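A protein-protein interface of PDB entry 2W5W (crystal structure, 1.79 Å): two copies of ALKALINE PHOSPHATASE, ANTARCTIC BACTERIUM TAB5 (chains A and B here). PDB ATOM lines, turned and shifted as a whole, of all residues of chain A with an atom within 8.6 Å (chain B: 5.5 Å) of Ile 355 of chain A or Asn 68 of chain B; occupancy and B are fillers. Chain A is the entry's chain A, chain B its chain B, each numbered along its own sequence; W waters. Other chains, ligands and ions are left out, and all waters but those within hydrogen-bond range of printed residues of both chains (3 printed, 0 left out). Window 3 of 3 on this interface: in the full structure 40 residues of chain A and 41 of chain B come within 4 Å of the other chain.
Among the printed residues, pairs that only touch across the chains: Lys 67 of chain A with Ile 355 of chain B, Ile 355 of chain A with Lys 67 of chain B, Gly 356 of chain A with Phe 66 of chain B, Ile 69 of chain A with Ile 69 of chain B, Leu 71 of chain A with Phe 345 of chain B, Gly 356 of chain A with Ile 69 of chain B and Ile 355 of chain A with Asn 68 of chain B.
Water W2 lies within hydrogen-bond range of the backbone carbonyl oxygen (O) of Phe 66 of chain B (2.7 Å), the backbone NH (N) of Ile 357 of chain A (2.9 Å) and the side-chain amino group (NZ) of Lys 67 of chain B (3.1 Å). Water W1 lies within hydrogen-bond range of O of Ile 69 of chain B (2.7 Å) and O of Ile 69 of chain A (2.8 Å). Water W3 bridges O of Ile 357 of chain A (2.8 Å) and NZ of Lys 67 of chain B (3.1 Å).
O of Lys 67 of chain B sits at hydrogen-bond distance from N of Gly 356 of chain A, 3.0 Å away.
Of the 11 printed residues of chain B, 6 touch a printed residue of chain A. Hydrophobic or aromatic side chains of chain B that line the printed part of chain A: Ile 69, Phe 345 and Ile 355. Hydrophobic or aromatic side chains of chain A that line the printed part of chain B: Ile 69, Leu 71 and Ile 355. Among the printed residues, 8 pairs touch across the chains. Among the printed residues, no Asp or Glu carboxylate lies within 4 Å of a Lys or Arg side-chain nitrogen of the other chain.
Lys 67 of chain A touches Ile 355 of chain B, and with the chains exchanged Ile 355 of chain A touches Lys 67 of chain B. Ile 69 of chain B touches its own counterpart, Ile 69 of chain A. Ile 355 of chain A touches Asn 68 of chain B, but with the chains exchanged Asn 68 of chain A does not touch Ile 355 of chain B (4.04 Å). Of the 8 pairs that touch across the chains among the printed residues, 3 have their exchanged pair printed and touching as well.
The backbone carbonyl oxygen (O) of Gly 356 of chain A is in hydrogen-bond range of the backbone NH (N) of Leu 71 of chain A (2.9 Å). The backbone NH of Tyr 358 of chain A sits at hydrogen-bond distance from the backbone carbonyl oxygen of Leu 71 of chain A. The backbone carbonyl oxygen of Asn 68 of chain B is in hydrogen-bond range of the backbone NH of Ala 346 of chain B (3.0 Å). The side-chain hydroxyl (OG) of Ser 351 of chain B is in hydrogen-bond range of the side-chain amide nitrogen (ND2) of Asn 68 of chain B (2.9 Å).
Printed residues of chain B within 4 Å of Ile 69 of chain A: Ile 69 (3.7 Å). Of the printed residues of chain B, Leu 71 of chain A touches Phe 345 (3.7 Å). Ile 355 of chain A touches two residues of chain B. Printed residues of chain B within 4 Å of Gly 356 of chain A: Phe 66 (3.4 Å), Lys 67 (3.0 Å) and Ile 69 (3.8 Å). Printed residues of chain A within 4 Å of Phe 66 of chain B: Gly 356 (3.4 Å). Asn 68 of chain B touches just one residue of chain A: Ile 355. No residue of chain A comes within 4 Å of Ala 346 of chain B. The nearest residue of chain B that does not touch Ile 355 of chain A is Ile 69 of chain B (5.2 Å).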
ATOM      1  N   LEU A  31      24.981   5.399   1.657  1.00  0.00           N
ATOM      2  CA  LEU A  31      23.547   5.243   1.455  1.00  0.00           C
ATOM      3  C   LEU A  31      22.793   5.840   2.635  1.00  0.00           C
ATOM      4  O   LEU A  31      23.397   6.217   3.642  1.00  0.00           O
ATOM      5  CB  LEU A  31      23.181   3.767   1.309  1.00  0.00           C
ATOM      6  CG  LEU A  31      23.874   2.987   0.194  1.00  0.00           C
ATOM      7  CD1 LEU A  31      23.383   1.549   0.177  1.00  0.00           C
ATOM      8  CD2 LEU A  31      23.640   3.657  -1.150  1.00  0.00           C
ATOM      9  N   LYS A  67      13.867  -1.185  -8.366  1.00  0.00           N
ATOM     10  CA  LYS A  67      15.033  -0.924  -9.218  1.00  0.00           C
ATOM     11  C   LYS A  67      16.251  -1.709  -8.744  1.00  0.00           C
ATOM     12  O   LYS A  67      16.985  -2.300  -9.550  1.00  0.00           O
ATOM     13  CB  LYS A  67      15.352   0.570  -9.250  1.00  0.00           C
ATOM     14  CG  LYS A  67      14.202   1.411  -9.768  1.00  0.00           C
ATOM     15  CD  LYS A  67      13.861   1.033 -11.212  1.00  0.00           C
ATOM     16  CE  LYS A  67      12.513   1.628 -11.628  1.00  0.00           C
ATOM     17  NZ  LYS A  67      12.017   1.041 -12.927  1.00  0.00           N
ATOM     18  N   ASN A  68      16.455  -1.740  -7.430  1.00  0.00           N
ATOM     19  CA  ASN A  68      17.636  -2.387  -6.887  1.00  0.00           C
ATOM     20  C   ASN A  68      17.398  -3.873  -6.702  1.00  0.00           C
ATOM     21  O   ASN A  68      16.517  -4.288  -5.939  1.00  0.00           O
ATOM     22  CB  ASN A  68      18.033  -1.728  -5.557  1.00  0.00           C
ATOM     23  CG  ASN A  68      18.461  -0.287  -5.752  1.00  0.00           C
ATOM     24  OD1 ASN A  68      19.248   0.016  -6.658  1.00  0.00           O
ATOM     25  ND2 ASN A  68      17.909   0.617  -4.948  1.00  0.00           N
ATOM     26  N   ILE A  69      18.201  -4.663  -7.404  1.00  0.00           N
ATOM     27  CA  ILE A  69      18.017  -6.109  -7.472  1.00  0.00           C
ATOM     28  C   ILE A  69      19.353  -6.768  -7.204  1.00  0.00           C
ATOM     29  O   ILE A  69      20.386  -6.306  -7.708  1.00  0.00           O
ATOM     30  CB  ILE A  69      17.453  -6.528  -8.864  1.00  0.00           C
ATOM     31  CG1 ILE A  69      16.067  -5.902  -9.051  1.00  0.00           C
ATOM     32  CG2 ILE A  69      17.385  -8.072  -8.982  1.00  0.00           C
ATOM     33  CD1 ILE A  69      15.476  -6.002 -10.478  1.00  0.00           C
ATOM     34  N   GLY A  70      19.329  -7.817  -6.385  1.00  0.00           N
ATOM     35  CA  GLY A  70      20.499  -8.648  -6.142  1.00  0.00           C
ATOM     36  C   GLY A  70      20.170 -10.121  -6.323  1.00  0.00           C
ATOM     37  O   GLY A  70      19.042 -10.468  -6.671  1.00  0.00           O
ATOM     38  N   LEU A  71      21.156 -10.986  -6.101  1.00  0.00           N
ATOM     39  CA  LEU A  71      20.953 -12.427  -6.176  1.00  0.00           C
ATOM     40  C   LEU A  71      21.630 -13.084  -4.975  1.00  0.00           C
ATOM     41  O   LEU A  71      22.757 -12.709  -4.614  1.00  0.00           O
ATOM     42  CB  LEU A  71      21.566 -12.996  -7.473  1.00  0.00           C
ATOM     43  CG  LEU A  71      20.991 -12.481  -8.783  1.00  0.00           C
ATOM     44  CD1 LEU A  71      21.912 -12.873  -9.956  1.00  0.00           C
ATOM     45  CD2 LEU A  71      19.560 -13.023  -8.991  1.00  0.00           C
ATOM     46  N   ILE A  72      20.954 -14.063  -4.357  1.00  0.00           N
ATOM     47  CA  ILE A  72      21.553 -14.802  -3.258  1.00  0.00           C
ATOM     48  C   ILE A  72      21.767 -16.286  -3.563  1.00  0.00           C
ATOM     49  O   ILE A  72      20.943 -16.941  -4.211  1.00  0.00           O
ATOM     50  CB  ILE A  72      20.758 -14.680  -1.920  1.00  0.00           C
ATOM     51  CG1 ILE A  72      19.265 -14.955  -2.128  1.00  0.00           C
ATOM     52  CG2 ILE A  72      20.947 -13.296  -1.306  1.00  0.00           C
ATOM     53  CD1 ILE A  72      18.480 -15.062  -0.781  1.00  0.00           C
ATOM     54  N   VAL A 344      16.812 -10.893  -5.096  1.00  0.00           N
ATOM     55  CA  VAL A 344      16.486 -10.061  -3.944  1.00  0.00           C
ATOM     56  C   VAL A 344      16.054  -8.714  -4.509  1.00  0.00           C
ATOM     57  O   VAL A 344      16.703  -8.192  -5.408  1.00  0.00           O
ATOM     58  CB  VAL A 344      17.728  -9.790  -3.070  1.00  0.00           C
ATOM     59  CG1 VAL A 344      17.338  -8.960  -1.847  1.00  0.00           C
ATOM     60  CG2 VAL A 344      18.384 -11.107  -2.642  1.00  0.00           C
ATOM     61  N   PHE A 345      14.950  -8.180  -4.012  1.00  0.00           N
ATOM     62  CA  PHE A 345      14.473  -6.863  -4.421  1.00  0.00           C
ATOM     63  C   PHE A 345      14.477  -5.935  -3.198  1.00  0.00           C
ATOM     64  O   PHE A 345      14.063  -6.338  -2.113  1.00  0.00           O
ATOM     65  CB  PHE A 345      13.047  -6.959  -4.972  1.00  0.00           C
ATOM     66  CG  PHE A 345      12.885  -7.986  -6.072  1.00  0.00           C
ATOM     67  CD1 PHE A 345      12.930  -7.597  -7.406  1.00  0.00           C
ATOM     68  CD2 PHE A 345      12.682  -9.332  -5.763  1.00  0.00           C
ATOM     69  CE1 PHE A 345      12.779  -8.526  -8.427  1.00  0.00           C
ATOM     70  CE2 PHE A 345      12.529 -10.288  -6.772  1.00  0.00           C
ATOM     71  CZ  PHE A 345      12.583  -9.888  -8.109  1.00  0.00           C
ATOM     72  N   ALA A 346      14.937  -4.704  -3.370  1.00  0.00           N
ATOM     73  CA  ALA A 346      14.972  -3.774  -2.247  1.00  0.00           C
ATOM     74  C   ALA A 346      14.537  -2.384  -2.684  1.00  0.00           C
ATOM     75  O   ALA A 346      14.959  -1.892  -3.740  1.00  0.00           O
ATOM     76  CB  ALA A 346      16.389  -3.725  -1.640  1.00  0.00           C
ATOM     77  N   GLY A 350      18.858   2.788   1.909  1.00  0.00           N
ATOM     78  CA  GLY A 350      19.773   1.665   2.025  1.00  0.00           C
ATOM     79  C   GLY A 350      19.568   0.567   0.991  1.00  0.00           C
ATOM     80  O   GLY A 350      20.262  -0.443   1.004  1.00  0.00           O
ATOM     81  N   SER A 351      18.607   0.743   0.095  1.00  0.00           N
ATOM     82  CA  SER A 351      18.267  -0.355  -0.819  1.00  0.00           C
ATOM     83  C   SER A 351      19.440  -0.757  -1.730  1.00  0.00           C
ATOM     84  O   SER A 351      19.531  -1.918  -2.148  1.00  0.00           O
ATOM     85  CB  SER A 351      17.014  -0.014  -1.640  1.00  0.00           C
ATOM     86  OG  SER A 351      17.248   1.150  -2.430  1.00  0.00           O
ATOM     87  N   GLU A 352      20.345   0.183  -2.017  1.00  0.00           N
ATOM     88  CA  GLU A 352      21.501  -0.117  -2.877  1.00  0.00           C
ATOM     89  C   GLU A 352      22.477  -1.120  -2.275  1.00  0.00           C
ATOM     90  O   GLU A 352      23.303  -1.695  -2.988  1.00  0.00           O
ATOM     91  CB  GLU A 352      22.237   1.170  -3.265  1.00  0.00           C
ATOM     92  CG  GLU A 352      21.411   2.006  -4.232  1.00  0.00           C
ATOM     93  CD  GLU A 352      21.833   3.458  -4.305  1.00  0.00           C
ATOM     94  OE1 GLU A 352      20.937   4.330  -4.230  1.00  0.00           O
ATOM     95  OE2 GLU A 352      23.047   3.726  -4.449  1.00  0.00           O
ATOM     96  N   GLU A 353      22.404  -1.312  -0.959  1.00  0.00           N
ATOM     97  CA  GLU A 353      23.279  -2.271  -0.275  1.00  0.00           C
ATOM     98  C   GLU A 353      22.976  -3.699  -0.725  1.00  0.00           C
ATOM     99  O   GLU A 353      23.801  -4.603  -0.577  1.00  0.00           O
ATOM    100  CB  GLU A 353      23.089  -2.165   1.251  1.00  0.00           C
ATOM    101  CG  GLU A 353      24.209  -2.805   2.054  1.00  0.00           C
ATOM    102  CD  GLU A 353      25.534  -2.121   1.767  1.00  0.00           C
ATOM    103  OE1 GLU A 353      25.526  -0.889   1.566  1.00  0.00           O
ATOM    104  OE2 GLU A 353      26.571  -2.808   1.731  1.00  0.00           O
ATOM    105  N   PHE A 354      21.804  -3.904  -1.304  1.00  0.00           N
ATOM    106  CA  PHE A 354      21.330  -5.258  -1.571  1.00  0.00           C
ATOM    107  C   PHE A 354      21.533  -5.758  -3.009  1.00  0.00           C
ATOM    108  O   PHE A 354      21.053  -6.825  -3.370  1.00  0.00           O
ATOM    109  CB  PHE A 354      19.862  -5.371  -1.161  1.00  0.00           C
ATOM    110  CG  PHE A 354      19.674  -5.215   0.318  1.00  0.00           C
ATOM    111  CD1 PHE A 354      19.604  -3.958   0.891  1.00  0.00           C
ATOM    112  CD2 PHE A 354      19.652  -6.326   1.145  1.00  0.00           C
ATOM    113  CE1 PHE A 354      19.473  -3.821   2.307  1.00  0.00           C
ATOM    114  CE2 PHE A 354      19.524  -6.197   2.539  1.00  0.00           C
ATOM    115  CZ  PHE A 354      19.440  -4.952   3.111  1.00  0.00           C
ATOM    116  N   ILE A 355      22.257  -4.991  -3.806  1.00  0.00           N
ATOM    117  CA  ILE A 355      22.538  -5.391  -5.188  1.00  0.00           C
ATOM    118  C   ILE A 355      23.762  -6.322  -5.256  1.00  0.00           C
ATOM    119  O   ILE A 355      24.353  -6.660  -4.234  1.00  0.00           O
ATOM    120  CB  ILE A 355      22.705  -4.144  -6.096  1.00  0.00           C
ATOM    121  CG1 ILE A 355      24.025  -3.426  -5.824  1.00  0.00           C
ATOM    122  CG2 ILE A 355      21.513  -3.168  -5.913  1.00  0.00           C
ATOM    123  CD1 ILE A 355      24.194  -2.174  -6.717  1.00  0.00           C
ATOM    124  N   GLY A 356      24.132  -6.765  -6.449  1.00  0.00           N
ATOM    125  CA  GLY A 356      25.214  -7.726  -6.568  1.00  0.00           C
ATOM    126  C   GLY A 356      24.802  -9.138  -6.188  1.00  0.00           C
ATOM    127  O   GLY A 356      23.619  -9.429  -6.023  1.00  0.00           O
ATOM    128  N   ILE A 357      25.786 -10.025  -6.088  1.00  0.00           N
ATOM    129  CA  ILE A 357      25.537 -11.434  -5.808  1.00  0.00           C
ATOM    130  C   ILE A 357      26.228 -11.770  -4.501  1.00  0.00           C
ATOM    131  O   ILE A 357      27.394 -11.422  -4.316  1.00  0.00           O
ATOM    132  CB  ILE A 357      26.112 -12.343  -6.927  1.00  0.00           C
ATOM    133  CG1 ILE A 357      25.528 -11.948  -8.286  1.00  0.00           C
ATOM    134  CG2 ILE A 357      25.803 -13.799  -6.629  1.00  0.00           C
ATOM    135  CD1 ILE A 357      26.027 -12.820  -9.440  1.00  0.00           C
ATOM    136  N   TYR A 358      25.524 -12.439  -3.595  1.00  0.00           N
ATOM    137  CA  TYR A 358      26.096 -12.724  -2.260  1.00  0.00           C
ATOM    138  C   TYR A 358      25.458 -13.954  -1.615  1.00  0.00           C
ATOM    139  O   TYR A 358      24.477 -14.472  -2.126  1.00  0.00           O
ATOM    140  CB  TYR A 358      25.977 -11.500  -1.349  1.00  0.00           C
ATOM    141  CG  TYR A 358      24.629 -10.784  -1.377  1.00  0.00           C
ATOM    142  CD1 TYR A 358      23.637 -11.097  -0.455  1.00  0.00           C
ATOM    143  CD2 TYR A 358      24.363  -9.788  -2.330  1.00  0.00           C
ATOM    144  CE1 TYR A 358      22.427 -10.443  -0.460  1.00  0.00           C
ATOM    145  CE2 TYR A 358      23.142  -9.136  -2.363  1.00  0.00           C
ATOM    146  CZ  TYR A 358      22.180  -9.464  -1.418  1.00  0.00           C
ATOM    147  OH  TYR A 358      20.959  -8.831  -1.428  1.00  0.00           O
ATOM    148  N   ILE A 363      22.124 -11.262   3.964  1.00  0.00           N
ATOM    149  CA  ILE A 363      20.920 -10.438   4.120  1.00  0.00           C
ATOM    150  C   ILE A 363      20.851  -9.847   5.544  1.00  0.00           C
ATOM    151  O   ILE A 363      20.544  -8.680   5.730  1.00  0.00           O
ATOM    152  CB  ILE A 363      19.641 -11.273   3.829  1.00  0.00           C
ATOM    153  CG1 ILE A 363      19.506 -11.552   2.318  1.00  0.00           C
ATOM    154  CG2 ILE A 363      18.398 -10.566   4.335  1.00  0.00           C
ATOM    155  CD1 ILE A 363      19.082 -10.352   1.509  1.00  0.00           C
ATOM    156  N   LYS A 366      23.591  -7.108   5.965  1.00  0.00           N
ATOM    157  CA  LYS A 366      23.235  -5.903   5.214  1.00  0.00           C
ATOM    158  C   LYS A 366      22.130  -5.104   5.908  1.00  0.00           C
ATOM    159  O   LYS A 366      22.175  -3.878   5.946  1.00  0.00           O
ATOM    160  CB  LYS A 366      22.826  -6.266   3.777  1.00  0.00           C
ATOM    161  CG  LYS A 366      24.003  -6.719   2.923  1.00  0.00           C
ATOM    162  CD  LYS A 366      23.547  -7.338   1.593  1.00  0.00           C
ATOM    163  CE  LYS A 366      24.737  -7.821   0.770  1.00  0.00           C
ATOM    164  NZ  LYS A 366      25.625  -6.687   0.354  1.00  0.00           N
ATOM    165  N   PHE B  66      29.545  -8.498 -10.993  1.00  0.00           N
ATOM    166  CA  PHE B  66      28.495  -7.523 -11.292  1.00  0.00           C
ATOM    167  C   PHE B  66      27.725  -7.095 -10.062  1.00  0.00           C
ATOM    168  O   PHE B  66      27.407  -7.914  -9.190  1.00  0.00           O
ATOM    169  CB  PHE B  66      27.465  -8.105 -12.280  1.00  0.00           C
ATOM    170  CG  PHE B  66      27.998  -8.319 -13.651  1.00  0.00           C
ATOM    171  CD1 PHE B  66      28.316  -9.591 -14.088  1.00  0.00           C
ATOM    172  CD2 PHE B  66      28.154  -7.246 -14.519  1.00  0.00           C
ATOM    173  CE1 PHE B  66      28.813  -9.787 -15.381  1.00  0.00           C
ATOM    174  CE2 PHE B  66      28.643  -7.428 -15.810  1.00  0.00           C
ATOM    175  CZ  PHE B  66      28.971  -8.694 -16.240  1.00  0.00           C
ATOM    176  N   LYS B  67      27.419  -5.805 -10.010  1.00  0.00           N
ATOM    177  CA  LYS B  67      26.580  -5.248  -8.964  1.00  0.00           C
ATOM    178  C   LYS B  67      25.228  -4.849  -9.558  1.00  0.00           C
ATOM    179  O   LYS B  67      24.171  -5.144  -9.002  1.00  0.00           O
ATOM    180  CB  LYS B  67      27.266  -4.020  -8.360  1.00  0.00           C
ATOM    181  CG  LYS B  67      28.636  -4.335  -7.775  1.00  0.00           C
ATOM    182  CD  LYS B  67      28.527  -5.467  -6.759  1.00  0.00           C
ATOM    183  CE  LYS B  67      29.894  -5.908  -6.229  1.00  0.00           C
ATOM    184  NZ  LYS B  67      29.735  -6.949  -5.162  1.00  0.00           N
ATOM    185  N   ASN B  68      25.261  -4.147 -10.681  1.00  0.00           N
ATOM    186  CA  ASN B  68      24.020  -3.690 -11.303  1.00  0.00           C
ATOM    187  C   ASN B  68      23.347  -4.812 -12.077  1.00  0.00           C
ATOM    188  O   ASN B  68      23.913  -5.343 -13.031  1.00  0.00           O
ATOM    189  CB  ASN B  68      24.288  -2.501 -12.210  1.00  0.00           C
ATOM    190  CG  ASN B  68      24.795  -1.297 -11.436  1.00  0.00           C
ATOM    191  OD1 ASN B  68      24.290  -0.987 -10.360  1.00  0.00           O
ATOM    192  ND2 ASN B  68      25.797  -0.617 -11.983  1.00  0.00           N
ATOM    193  N   ILE B  69      22.139  -5.155 -11.642  1.00  0.00           N
ATOM    194  CA  ILE B  69      21.402  -6.295 -12.164  1.00  0.00           C
ATOM    195  C   ILE B  69      19.978  -5.853 -12.472  1.00  0.00           C
ATOM    196  O   ILE B  69      19.372  -5.098 -11.697  1.00  0.00           O
ATOM    197  CB  ILE B  69      21.411  -7.446 -11.113  1.00  0.00           C
ATOM    198  CG1 ILE B  69      22.839  -7.963 -10.934  1.00  0.00           C
ATOM    199  CG2 ILE B  69      20.439  -8.583 -11.515  1.00  0.00           C
ATOM    200  CD1 ILE B  69      23.030  -8.899  -9.723  1.00  0.00           C
ATOM    201  N   GLY B  70      19.455  -6.276 -13.632  1.00  0.00           N
ATOM    202  CA  GLY B  70      18.068  -6.039 -13.987  1.00  0.00           C
ATOM    203  C   GLY B  70      17.398  -7.332 -14.433  1.00  0.00           C
ATOM    204  O   GLY B  70      18.020  -8.394 -14.392  1.00  0.00           O
ATOM    205  N   VAL B 344      19.748  -9.522 -16.285  1.00  0.00           N
ATOM    206  CA  VAL B 344      20.631  -8.671 -17.055  1.00  0.00           C
ATOM    207  C   VAL B 344      21.696  -8.188 -16.086  1.00  0.00           C
ATOM    208  O   VAL B 344      21.376  -7.747 -14.975  1.00  0.00           O
ATOM    209  CB  VAL B 344      19.896  -7.416 -17.547  1.00  0.00           C
ATOM    210  CG1 VAL B 344      20.879  -6.474 -18.291  1.00  0.00           C
ATOM    211  CG2 VAL B 344      18.708  -7.808 -18.450  1.00  0.00           C
ATOM    212  N   PHE B 345      22.955  -8.250 -16.501  1.00  0.00           N
ATOM    213  CA  PHE B 345      24.062  -7.796 -15.665  1.00  0.00           C
ATOM    214  C   PHE B 345      24.778  -6.695 -16.429  1.00  0.00           C
ATOM    215  O   PHE B 345      24.980  -6.813 -17.632  1.00  0.00           O
ATOM    216  CB  PHE B 345      25.059  -8.943 -15.391  1.00  0.00           C
ATOM    217  CG  PHE B 345      24.428 -10.176 -14.788  1.00  0.00           C
ATOM    218  CD1 PHE B 345      24.369 -10.343 -13.411  1.00  0.00           C
ATOM    219  CD2 PHE B 345      23.858 -11.135 -15.597  1.00  0.00           C
ATOM    220  CE1 PHE B 345      23.781 -11.470 -12.852  1.00  0.00           C
ATOM    221  CE2 PHE B 345      23.270 -12.274 -15.047  1.00  0.00           C
ATOM    222  CZ  PHE B 345      23.236 -12.435 -13.662  1.00  0.00           C
ATOM    223  N   ALA B 346      25.197  -5.639 -15.748  1.00  0.00           N
ATOM    224  CA  ALA B 346      25.916  -4.581 -16.458  1.00  0.00           C
ATOM    225  C   ALA B 346      27.014  -3.982 -15.605  1.00  0.00           C
ATOM    226  O   ALA B 346      26.825  -3.747 -14.404  1.00  0.00           O
ATOM    227  CB  ALA B 346      24.940  -3.487 -16.935  1.00  0.00           C
ATOM    228  N   SER B 351      26.083   1.688 -16.631  1.00  0.00           N
ATOM    229  CA  SER B 351      25.521   0.391 -16.244  1.00  0.00           C
ATOM    230  C   SER B 351      24.295   0.498 -15.348  1.00  0.00           C
ATOM    231  O   SER B 351      23.455  -0.408 -15.342  1.00  0.00           O
ATOM    232  CB  SER B 351      26.584  -0.527 -15.610  1.00  0.00           C
ATOM    233  OG  SER B 351      27.159   0.075 -14.461  1.00  0.00           O
ATOM    234  N   GLU B 352      24.169   1.599 -14.605  1.00  0.00           N
ATOM    235  CA  GLU B 352      23.019   1.774 -13.708  1.00  0.00           C
ATOM    236  C   GLU B 352      21.696   1.878 -14.494  1.00  0.00           C
ATOM    237  O   GLU B 352      20.616   1.679 -13.951  1.00  0.00           O
ATOM    238  CB  GLU B 352      23.207   3.021 -12.827  1.00  0.00           C
ATOM    239  CG  GLU B 352      24.496   3.022 -11.977  1.00  0.00           C
ATOM    240  CD  GLU B 352      25.780   3.277 -12.783  1.00  0.00           C
ATOM    241  OE1 GLU B 352      25.713   3.803 -13.919  1.00  0.00           O
ATOM    242  OE2 GLU B 352      26.873   2.952 -12.267  1.00  0.00           O
ATOM    243  N   ILE B 355      19.255  -1.508 -14.523  1.00  0.00           N
ATOM    244  CA  ILE B 355      18.640  -2.145 -13.351  1.00  0.00           C
ATOM    245  C   ILE B 355      17.116  -2.119 -13.476  1.00  0.00           C
ATOM    246  O   ILE B 355      16.591  -1.607 -14.452  1.00  0.00           O
ATOM    247  CB  ILE B 355      19.085  -1.465 -12.038  1.00  0.00           C
ATOM    248  CG1 ILE B 355      18.570  -0.025 -11.935  1.00  0.00           C
ATOM    249  CG2 ILE B 355      20.625  -1.503 -11.922  1.00  0.00           C
ATOM    250  CD1 ILE B 355      19.001   0.692 -10.631  1.00  0.00           C
HETATM  251  O   HOH W   1      20.465  -4.111  -9.376  1.00  0.00           O
HETATM  252  O   HOH W   2      28.353  -9.027  -6.966  1.00  0.00           O
HETATM  253  O   HOH W   3      28.264  -8.972  -3.391  1.00  0.00           O
